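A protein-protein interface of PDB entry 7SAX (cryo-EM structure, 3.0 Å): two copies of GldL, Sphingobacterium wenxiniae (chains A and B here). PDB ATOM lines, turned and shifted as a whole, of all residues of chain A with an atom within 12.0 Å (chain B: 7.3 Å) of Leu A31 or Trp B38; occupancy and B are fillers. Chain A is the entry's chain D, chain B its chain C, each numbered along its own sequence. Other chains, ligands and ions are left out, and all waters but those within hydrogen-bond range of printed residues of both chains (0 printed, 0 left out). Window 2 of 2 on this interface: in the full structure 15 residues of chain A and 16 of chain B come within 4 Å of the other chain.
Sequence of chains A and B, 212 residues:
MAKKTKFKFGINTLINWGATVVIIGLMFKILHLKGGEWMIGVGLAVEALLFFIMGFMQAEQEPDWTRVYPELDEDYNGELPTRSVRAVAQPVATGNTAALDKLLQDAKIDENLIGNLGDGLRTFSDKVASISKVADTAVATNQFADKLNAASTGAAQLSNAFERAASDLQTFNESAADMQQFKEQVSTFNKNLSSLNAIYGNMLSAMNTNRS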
ATOM      1  N   VAL A  22     -11.163 -10.541   5.828  1.00  0.00           N
ATOM      2  CA  VAL A  22     -10.698 -10.757   7.196  1.00  0.00           C
ATOM      3  C   VAL A  22     -11.682 -11.622   7.964  1.00  0.00           C
ATOM      4  O   VAL A  22     -11.289 -12.503   8.731  1.00  0.00           O
ATOM      5  CB  VAL A  22     -10.478  -9.419   7.917  1.00  0.00           C
ATOM      6  CG1 VAL A  22      -9.941  -9.667   9.304  1.00  0.00           C
ATOM      7  CG2 VAL A  22      -9.546  -8.553   7.145  1.00  0.00           C
ATOM      8  N   ILE A  23     -12.978 -11.365   7.793  1.00  0.00           N
ATOM      9  CA  ILE A  23     -13.985 -12.084   8.562  1.00  0.00           C
ATOM     10  C   ILE A  23     -14.116 -13.520   8.089  1.00  0.00           C
ATOM     11  O   ILE A  23     -14.386 -14.419   8.890  1.00  0.00           O
ATOM     12  CB  ILE A  23     -15.319 -11.333   8.503  1.00  0.00           C
ATOM     13  CG1 ILE A  23     -15.150  -9.973   9.152  1.00  0.00           C
ATOM     14  CG2 ILE A  23     -16.376 -12.084   9.242  1.00  0.00           C
ATOM     15  CD1 ILE A  23     -16.412  -9.278   9.356  1.00  0.00           C
ATOM     16  N   ILE A  24     -13.931 -13.771   6.795  1.00  0.00           N
ATOM     17  CA  ILE A  24     -13.873 -15.152   6.328  1.00  0.00           C
ATOM     18  C   ILE A  24     -12.674 -15.859   6.939  1.00  0.00           C
ATOM     19  O   ILE A  24     -12.755 -17.026   7.335  1.00  0.00           O
ATOM     20  CB  ILE A  24     -13.846 -15.199   4.792  1.00  0.00           C
ATOM     21  CG1 ILE A  24     -15.226 -14.871   4.239  1.00  0.00           C
ATOM     22  CG2 ILE A  24     -13.420 -16.557   4.310  1.00  0.00           C
ATOM     23  CD1 ILE A  24     -15.294 -14.887   2.745  1.00  0.00           C
ATOM     24  N   GLY A  25     -11.547 -15.159   7.046  1.00  0.00           N
ATOM     25  CA  GLY A  25     -10.407 -15.734   7.737  1.00  0.00           C
ATOM     26  C   GLY A  25     -10.703 -16.040   9.192  1.00  0.00           C
ATOM     27  O   GLY A  25     -10.291 -17.075   9.716  1.00  0.00           O
ATOM     28  N   LEU A  26     -11.415 -15.136   9.865  1.00  0.00           N
ATOM     29  CA  LEU A  26     -11.780 -15.352  11.263  1.00  0.00           C
ATOM     30  C   LEU A  26     -12.691 -16.559  11.414  1.00  0.00           C
ATOM     31  O   LEU A  26     -12.538 -17.351  12.348  1.00  0.00           O
ATOM     32  CB  LEU A  26     -12.464 -14.111  11.829  1.00  0.00           C
ATOM     33  CG  LEU A  26     -11.691 -12.801  11.873  1.00  0.00           C
ATOM     34  CD1 LEU A  26     -12.593 -11.682  12.326  1.00  0.00           C
ATOM     35  CD2 LEU A  26     -10.504 -12.925  12.783  1.00  0.00           C
ATOM     36  N   MET A  27     -13.658 -16.705  10.512  1.00  0.00           N
ATOM     37  CA  MET A  27     -14.527 -17.873  10.525  1.00  0.00           C
ATOM     38  C   MET A  27     -13.729 -19.150  10.315  1.00  0.00           C
ATOM     39  O   MET A  27     -13.988 -20.166  10.965  1.00  0.00           O
ATOM     40  CB  MET A  27     -15.597 -17.735   9.449  1.00  0.00           C
ATOM     41  CG  MET A  27     -16.344 -19.005   9.166  1.00  0.00           C
ATOM     42  SD  MET A  27     -17.524 -18.792   7.835  1.00  0.00           S
ATOM     43  CE  MET A  27     -16.759 -19.753   6.542  1.00  0.00           C
ATOM     44  N   PHE A  28     -12.760 -19.121   9.400  1.00  0.00           N
ATOM     45  CA  PHE A  28     -11.922 -20.292   9.183  1.00  0.00           C
ATOM     46  C   PHE A  28     -11.082 -20.615  10.406  1.00  0.00           C
ATOM     47  O   PHE A  28     -10.815 -21.786  10.679  1.00  0.00           O
ATOM     48  CB  PHE A  28     -11.018 -20.079   7.977  1.00  0.00           C
ATOM     49  CG  PHE A  28     -11.663 -20.417   6.670  1.00  0.00           C
ATOM     50  CD1 PHE A  28     -13.011 -20.216   6.477  1.00  0.00           C
ATOM     51  CD2 PHE A  28     -10.920 -20.943   5.639  1.00  0.00           C
ATOM     52  CE1 PHE A  28     -13.600 -20.527   5.282  1.00  0.00           C
ATOM     53  CE2 PHE A  28     -11.505 -21.251   4.441  1.00  0.00           C
ATOM     54  CZ  PHE A  28     -12.847 -21.044   4.263  1.00  0.00           C
ATOM     55  N   LYS A  29     -10.636 -19.596  11.135  1.00  0.00           N
ATOM     56  CA  LYS A  29      -9.856 -19.843  12.342  1.00  0.00           C
ATOM     57  C   LYS A  29     -10.726 -20.404  13.459  1.00  0.00           C
ATOM     58  O   LYS A  29     -10.289 -21.282  14.210  1.00  0.00           O
ATOM     59  CB  LYS A  29      -9.167 -18.559  12.790  1.00  0.00           C
ATOM     60  CG  LYS A  29      -8.515 -18.654  14.147  1.00  0.00           C
ATOM     61  CD  LYS A  29      -7.457 -17.596  14.325  1.00  0.00           C
ATOM     62  CE  LYS A  29      -7.001 -17.532  15.764  1.00  0.00           C
ATOM     63  NZ  LYS A  29      -6.481 -18.833  16.251  1.00  0.00           N
ATOM     64  N   ILE A  30     -11.954 -19.900  13.594  1.00  0.00           N
ATOM     65  CA  ILE A  30     -12.848 -20.367  14.648  1.00  0.00           C
ATOM     66  C   ILE A  30     -13.339 -21.780  14.367  1.00  0.00           C
ATOM     67  O   ILE A  30     -13.446 -22.607  15.279  1.00  0.00           O
ATOM     68  CB  ILE A  30     -14.015 -19.382  14.834  1.00  0.00           C
ATOM     69  CG1 ILE A  30     -13.554 -18.171  15.635  1.00  0.00           C
ATOM     70  CG2 ILE A  30     -15.196 -20.048  15.485  1.00  0.00           C
ATOM     71  CD1 ILE A  30     -14.615 -17.155  15.847  1.00  0.00           C
ATOM     72  N   LEU A  31     -13.646 -22.085  13.114  1.00  0.00           N
ATOM     73  CA  LEU A  31     -14.114 -23.410  12.742  1.00  0.00           C
ATOM     74  C   LEU A  31     -12.978 -24.382  12.477  1.00  0.00           C
ATOM     75  O   LEU A  31     -13.237 -25.512  12.054  1.00  0.00           O
ATOM     76  CB  LEU A  31     -15.017 -23.319  11.514  1.00  0.00           C
ATOM     77  CG  LEU A  31     -16.293 -22.518  11.742  1.00  0.00           C
ATOM     78  CD1 LEU A  31     -17.124 -22.456  10.485  1.00  0.00           C
ATOM     79  CD2 LEU A  31     -17.081 -23.138  12.862  1.00  0.00           C
ATOM     80  N   HIS A  32     -11.734 -23.967  12.703  1.00  0.00           N
ATOM     81  CA  HIS A  32     -10.565 -24.838  12.587  1.00  0.00           C
ATOM     82  C   HIS A  32     -10.421 -25.413  11.185  1.00  0.00           C
ATOM     83  O   HIS A  32     -10.002 -26.556  11.004  1.00  0.00           O
ATOM     84  CB  HIS A  32     -10.608 -25.954  13.625  1.00  0.00           C
ATOM     85  CG  HIS A  32     -10.800 -25.458  15.019  1.00  0.00           C
ATOM     86  ND1 HIS A  32     -12.021 -25.484  15.653  1.00  0.00           N
ATOM     87  CD2 HIS A  32      -9.930 -24.904  15.893  1.00  0.00           C
ATOM     88  CE1 HIS A  32     -11.894 -24.975  16.864  1.00  0.00           C
ATOM     89  NE2 HIS A  32     -10.635 -24.615  17.034  1.00  0.00           N
ATOM     90  N   LEU A  33     -10.762 -24.613  10.183  1.00  0.00           N
ATOM     91  CA  LEU A  33     -10.496 -24.987   8.807  1.00  0.00           C
ATOM     92  C   LEU A  33      -9.024 -24.723   8.494  1.00  0.00           C
ATOM     93  O   LEU A  33      -8.276 -24.185   9.314  1.00  0.00           O
ATOM     94  CB  LEU A  33     -11.438 -24.240   7.870  1.00  0.00           C
ATOM     95  CG  LEU A  33     -12.905 -24.365   8.289  1.00  0.00           C
ATOM     96  CD1 LEU A  33     -13.814 -23.627   7.338  1.00  0.00           C
ATOM     97  CD2 LEU A  33     -13.307 -25.818   8.386  1.00  0.00           C
ATOM     98  N   LYS A  34      -8.593 -25.106   7.294  1.00  0.00           N
ATOM     99  CA  LYS A  34      -7.164 -25.115   6.999  1.00  0.00           C
ATOM    100  C   LYS A  34      -6.610 -23.708   6.794  1.00  0.00           C
ATOM    101  O   LYS A  34      -5.802 -23.227   7.593  1.00  0.00           O
ATOM    102  CB  LYS A  34      -6.890 -25.984   5.772  1.00  0.00           C
ATOM    103  CG  LYS A  34      -5.457 -25.905   5.269  1.00  0.00           C
ATOM    104  CD  LYS A  34      -4.504 -26.665   6.170  1.00  0.00           C
ATOM    105  CE  LYS A  34      -4.264 -28.075   5.656  1.00  0.00           C
ATOM    106  NZ  LYS A  34      -3.044 -28.691   6.259  1.00  0.00           N
ATOM    107  N   GLY A  35      -7.035 -23.029   5.733  1.00  0.00           N
ATOM    108  CA  GLY A  35      -6.402 -21.779   5.364  1.00  0.00           C
ATOM    109  C   GLY A  35      -6.947 -20.556   6.069  1.00  0.00           C
ATOM    110  O   GLY A  35      -7.453 -19.637   5.421  1.00  0.00           O
ATOM    111  N   GLY A  36      -6.829 -20.517   7.391  1.00  0.00           N
ATOM    112  CA  GLY A  36      -7.441 -19.453   8.160  1.00  0.00           C
ATOM    113  C   GLY A  36      -6.570 -18.240   8.403  1.00  0.00           C
ATOM    114  O   GLY A  36      -6.984 -17.114   8.126  1.00  0.00           O
ATOM    115  N   GLU A  37      -5.360 -18.454   8.923  1.00  0.00           N
ATOM    116  CA  GLU A  37      -4.484 -17.334   9.247  1.00  0.00           C
ATOM    117  C   GLU A  37      -3.975 -16.604   8.014  1.00  0.00           C
ATOM    118  O   GLU A  37      -3.635 -15.421   8.111  1.00  0.00           O
ATOM    119  CB  GLU A  37      -3.309 -17.809  10.097  1.00  0.00           C
ATOM    120  CG  GLU A  37      -3.711 -18.277  11.482  1.00  0.00           C
ATOM    121  CD  GLU A  37      -4.213 -19.705  11.507  1.00  0.00           C
ATOM    122  OE1 GLU A  37      -4.192 -20.363  10.447  1.00  0.00           O
ATOM    123  OE2 GLU A  37      -4.627 -20.174  12.588  1.00  0.00           O
ATOM    124  N   MET A  39      -5.718 -15.731   5.261  1.00  0.00           N
ATOM    125  CA  MET A  39      -6.677 -14.679   4.946  1.00  0.00           C
ATOM    126  C   MET A  39      -6.729 -13.624   6.035  1.00  0.00           C
ATOM    127  O   MET A  39      -6.867 -12.438   5.737  1.00  0.00           O
ATOM    128  CB  MET A  39      -8.071 -15.250   4.702  1.00  0.00           C
ATOM    129  CG  MET A  39      -8.182 -16.106   3.474  1.00  0.00           C
ATOM    130  SD  MET A  39      -9.860 -16.674   3.224  1.00  0.00           S
ATOM    131  CE  MET A  39      -9.961 -17.903   4.503  1.00  0.00           C
ATOM    132  N   ILE A  40      -6.607 -14.023   7.301  1.00  0.00           N
ATOM    133  CA  ILE A  40      -6.571 -13.032   8.373  1.00  0.00           C
ATOM    134  C   ILE A  40      -5.433 -12.054   8.137  1.00  0.00           C
ATOM    135  O   ILE A  40      -5.638 -10.838   8.100  1.00  0.00           O
ATOM    136  CB  ILE A  40      -6.433 -13.713   9.745  1.00  0.00           C
ATOM    137  CG1 ILE A  40      -7.669 -14.531  10.076  1.00  0.00           C
ATOM    138  CG2 ILE A  40      -6.218 -12.677  10.814  1.00  0.00           C
ATOM    139  CD1 ILE A  40      -7.668 -15.052  11.479  1.00  0.00           C
ATOM    140  N   GLY B  25     -26.025 -16.281  17.648  1.00  0.00           N
ATOM    141  CA  GLY B  25     -24.693 -16.842  17.802  1.00  0.00           C
ATOM    142  C   GLY B  25     -23.953 -16.270  18.994  1.00  0.00           C
ATOM    143  O   GLY B  25     -23.335 -17.004  19.763  1.00  0.00           O
ATOM    144  N   LYS B  29     -22.651 -18.117  22.383  1.00  0.00           N
ATOM    145  CA  LYS B  29     -21.244 -18.045  22.752  1.00  0.00           C
ATOM    146  C   LYS B  29     -21.051 -17.529  24.173  1.00  0.00           C
ATOM    147  O   LYS B  29     -20.237 -18.072  24.923  1.00  0.00           O
ATOM    148  CB  LYS B  29     -20.495 -17.159  21.763  1.00  0.00           C
ATOM    149  CG  LYS B  29     -19.011 -17.112  21.987  1.00  0.00           C
ATOM    150  CD  LYS B  29     -18.311 -18.228  21.261  1.00  0.00           C
ATOM    151  CE  LYS B  29     -16.819 -18.155  21.474  1.00  0.00           C
ATOM    152  NZ  LYS B  29     -16.405 -18.870  22.712  1.00  0.00           N
ATOM    153  N   LYS B  34     -24.739 -25.185  24.145  1.00  0.00           N
ATOM    154  CA  LYS B  34     -24.161 -26.373  23.521  1.00  0.00           C
ATOM    155  C   LYS B  34     -23.600 -26.093  22.135  1.00  0.00           C
ATOM    156  O   LYS B  34     -22.510 -26.564  21.795  1.00  0.00           O
ATOM    157  CB  LYS B  34     -25.199 -27.485  23.449  1.00  0.00           C
ATOM    158  CG  LYS B  34     -24.671 -28.743  22.807  1.00  0.00           C
ATOM    159  CD  LYS B  34     -23.620 -29.397  23.654  1.00  0.00           C
ATOM    160  CE  LYS B  34     -23.226 -30.727  23.060  1.00  0.00           C
ATOM    161  NZ  LYS B  34     -22.547 -30.543  21.752  1.00  0.00           N
ATOM    162  N   GLY B  35     -24.323 -25.352  21.315  1.00  0.00           N
ATOM    163  CA  GLY B  35     -23.843 -25.097  19.975  1.00  0.00           C
ATOM    164  C   GLY B  35     -23.032 -23.835  19.802  1.00  0.00           C
ATOM    165  O   GLY B  35     -22.734 -23.459  18.665  1.00  0.00           O
ATOM    166  N   GLY B  36     -22.658 -23.167  20.889  1.00  0.00           N
ATOM    167  CA  GLY B  36     -22.022 -21.871  20.785  1.00  0.00           C
ATOM    168  C   GLY B  36     -20.640 -21.888  20.179  1.00  0.00           C
ATOM    169  O   GLY B  36     -20.108 -20.817  19.877  1.00  0.00           O
ATOM    170  N   GLU B  37     -20.050 -23.063  19.991  1.00  0.00           N
ATOM    171  CA  GLU B  37     -18.700 -23.138  19.452  1.00  0.00           C
ATOM    172  C   GLU B  37     -18.648 -22.838  17.961  1.00  0.00           C
ATOM    173  O   GLU B  37     -17.679 -22.234  17.495  1.00  0.00           O
ATOM    174  CB  GLU B  37     -18.106 -24.515  19.731  1.00  0.00           C
ATOM    175  CG  GLU B  37     -17.974 -24.843  21.207  1.00  0.00           C
ATOM    176  CD  GLU B  37     -19.185 -25.556  21.764  1.00  0.00           C
ATOM    177  OE1 GLU B  37     -19.726 -26.438  21.065  1.00  0.00           O
ATOM    178  OE2 GLU B  37     -19.592 -25.242  22.904  1.00  0.00           O
ATOM    179  N   TRP B  38     -19.663 -23.254  17.200  1.00  0.00           N
ATOM    180  CA  TRP B  38     -19.700 -23.027  15.763  1.00  0.00           C
ATOM    181  C   TRP B  38     -20.790 -22.069  15.319  1.00  0.00           C
ATOM    182  O   TRP B  38     -20.731 -21.576  14.188  1.00  0.00           O
ATOM    183  CB  TRP B  38     -19.887 -24.353  15.017  1.00  0.00           C
ATOM    184  CG  TRP B  38     -21.072 -25.129  15.474  1.00  0.00           C
ATOM    185  CD1 TRP B  38     -21.099 -26.086  16.439  1.00  0.00           C
ATOM    186  CD2 TRP B  38     -22.407 -25.017  14.981  1.00  0.00           C
ATOM    187  NE1 TRP B  38     -22.370 -26.575  16.581  1.00  0.00           N
ATOM    188  CE2 TRP B  38     -23.193 -25.933  15.696  1.00  0.00           C
ATOM    189  CE3 TRP B  38     -23.015 -24.227  14.008  1.00  0.00           C
ATOM    190  CZ2 TRP B  38     -24.551 -26.082  15.469  1.00  0.00           C
ATOM    191  CZ3 TRP B  38     -24.360 -24.377  13.784  1.00  0.00           C
ATOM    192  CH2 TRP B  38     -25.115 -25.295  14.509  1.00  0.00           C
ATOM    193  N   MET B  39     -21.791 -21.805  16.154  1.00  0.00           N
ATOM    194  CA  MET B  39     -22.751 -20.775  15.791  1.00  0.00           C
ATOM    195  C   MET B  39     -22.102 -19.406  15.740  1.00  0.00           C
ATOM    196  O   MET B  39     -22.573 -18.537  15.004  1.00  0.00           O
ATOM    197  CB  MET B  39     -23.935 -20.774  16.749  1.00  0.00           C
ATOM    198  CG  MET B  39     -24.766 -22.022  16.641  1.00  0.00           C
ATOM    199  SD  MET B  39     -26.121 -22.090  17.803  1.00  0.00           S
ATOM    200  CE  MET B  39     -27.171 -20.829  17.106  1.00  0.00           C
ATOM    201  N   ILE B  40     -21.014 -19.203  16.479  1.00  0.00           N
ATOM    202  CA  ILE B  40     -20.268 -17.964  16.318  1.00  0.00           C
ATOM    203  C   ILE B  40     -19.627 -17.910  14.939  1.00  0.00           C
ATOM    204  O   ILE B  40     -19.548 -16.840  14.332  1.00  0.00           O
ATOM    205  CB  ILE B  40     -19.241 -17.799  17.453  1.00  0.00           C
ATOM    206  CG1 ILE B  40     -18.770 -16.351  17.520  1.00  0.00           C
ATOM    207  CG2 ILE B  40     -18.074 -18.743  17.289  1.00  0.00           C
ATOM    208  CD1 ILE B  40     -19.869 -15.387  17.847  1.00  0.00           C
ATOM    209  N   GLY B  41     -19.186 -19.051  14.407  1.00  0.00           N
ATOM    210  CA  GLY B  41     -18.681 -19.070  13.044  1.00  0.00           C
ATOM    211  C   GLY B  41     -19.765 -18.810  12.017  1.00  0.00           C
ATOM    212  O   GLY B  41     -19.530 -18.151  11.005  1.00  0.00           O
ATOM    213  N   VAL B  42     -20.964 -19.337  12.256  1.00  0.00           N
ATOM    214  CA  VAL B  42     -22.084 -19.051  11.359  1.00  0.00           C
ATOM    215  C   VAL B  42     -22.421 -17.565  11.382  1.00  0.00           C
ATOM    216  O   VAL B  42     -22.654 -16.946  10.336  1.00  0.00           O
ATOM    217  CB  VAL B  42     -23.303 -19.912  11.730  1.00  0.00           C
ATOM    218  CG1 VAL B  42     -24.530 -19.428  10.997  1.00  0.00           C
ATOM    219  CG2 VAL B  42     -23.031 -21.360  11.403  1.00  0.00           C
ATOM    220  N   GLY B  43     -22.454 -16.969  12.572  1.00  0.00           N
ATOM    221  CA  GLY B  43     -22.661 -15.536  12.669  1.00  0.00           C
ATOM    222  C   GLY B  43     -21.556 -14.730  12.019  1.00  0.00           C
ATOM    223  O   GLY B  43     -21.813 -13.673  11.450  1.00  0.00           O
ATOM    224  N   LEU B  44     -20.316 -15.215  12.094  1.00  0.00           N
ATOM    225  CA  LEU B  44     -19.218 -14.553  11.399  1.00  0.00           C
ATOM    226  C   LEU B  44     -19.382 -14.637   9.888  1.00  0.00           C
ATOM    227  O   LEU B  44     -19.079 -13.680   9.174  1.00  0.00           O
ATOM    228  CB  LEU B  44     -17.885 -15.160  11.819  1.00  0.00           C
ATOM    229  CG  LEU B  44     -17.162 -14.530  13.002  1.00  0.00           C
ATOM    230  CD1 LEU B  44     -15.828 -15.194  13.175  1.00  0.00           C
ATOM    231  CD2 LEU B  44     -16.983 -13.049  12.797  1.00  0.00           C
ATOM    232  N   ALA B  45     -19.846 -15.778   9.380  1.00  0.00           N
ATOM    233  CA  ALA B  45     -20.142 -15.882   7.954  1.00  0.00           C
ATOM    234  C   ALA B  45     -21.212 -14.884   7.551  1.00  0.00           C
ATOM    235  O   ALA B  45     -21.090 -14.205   6.524  1.00  0.00           O
ATOM    236  CB  ALA B  45     -20.592 -17.296   7.608  1.00  0.00           C
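O of Ile A30 lies within hydrogen-bond range of ND1 of His A32, at 3.2 Å.
Ile A23 touches Leu B44 (CG2 to O, 3.1 Å).
Leu B44 touches Leu A26.
Met A27 touches Gly B41.
N of Met A27 touches CD1 of Leu B44, at 3.8 Å.
Met A27 touches Ala B45 (SD to CB, 3.4 Å).
Glu B37 touches Ile A30 (O to CG2, 3.9 Å).
Ile B40 touches Ile A30 (CG2 to CG2, 3.6 Å).
CD1 of Ile A30 touches CD1 of Leu B44, at 3.5 Å.
Trp B38 touches Leu A31.
Of chain B, only Trp B38 (3.7 Å) comes within 4 Å of Leu A31.
Of chain A, only Leu A31 (3.7 Å) comes within 4 Å of Trp B38.
No residue of chain A comes within 4 Å of Gly B35.
No residue of chain A comes within 4 Å of Gly B36.
Of the printed residues of chain A, Gly B41 touches Met A27 (3.8 Å).
Printed residues of chain B within 4 Å of Ile A30: Glu B37 (3.9 Å), Ile B40 (3.6 Å) and Leu B44 (3.5 Å).
Of the printed residues of chain B, Ile A23 touches Leu B44.
His A32 touches none of the printed residues of chain B.
Leu A33 touches none of the printed residues of chain B.
The nearest residue of chain B that does not touch Leu A31 is Gly B41 (4.4 Å).
The nearest residue of chain A that does not touch Trp B38 is Ile A30 (5.4 Å).
Hydrophobic or aromatic side chains of chain A within 4 Å of the printed part of chain B: Ile A23, Leu A26, Met A27, Ile A30 and Leu A31.
Of the 14 printed residues of chain B, 6 touch a printed residue of chain A.
Printed residues of chain B that touch a printed residue of chain A: Glu B37, Trp B38, Ile B40, Gly B41, Leu B44 and Ala B45.
Hydrophobic or aromatic side chains of chain B within 4 Å of the printed part of chain A: Trp B38, Ile B40, Leu B44 and Ala B45.
Among the printed residues, no Asp or Glu carboxylate lies within 4 Å of a Lys or Arg side-chain nitrogen of the other chain.
8 positions are printed for both chains.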
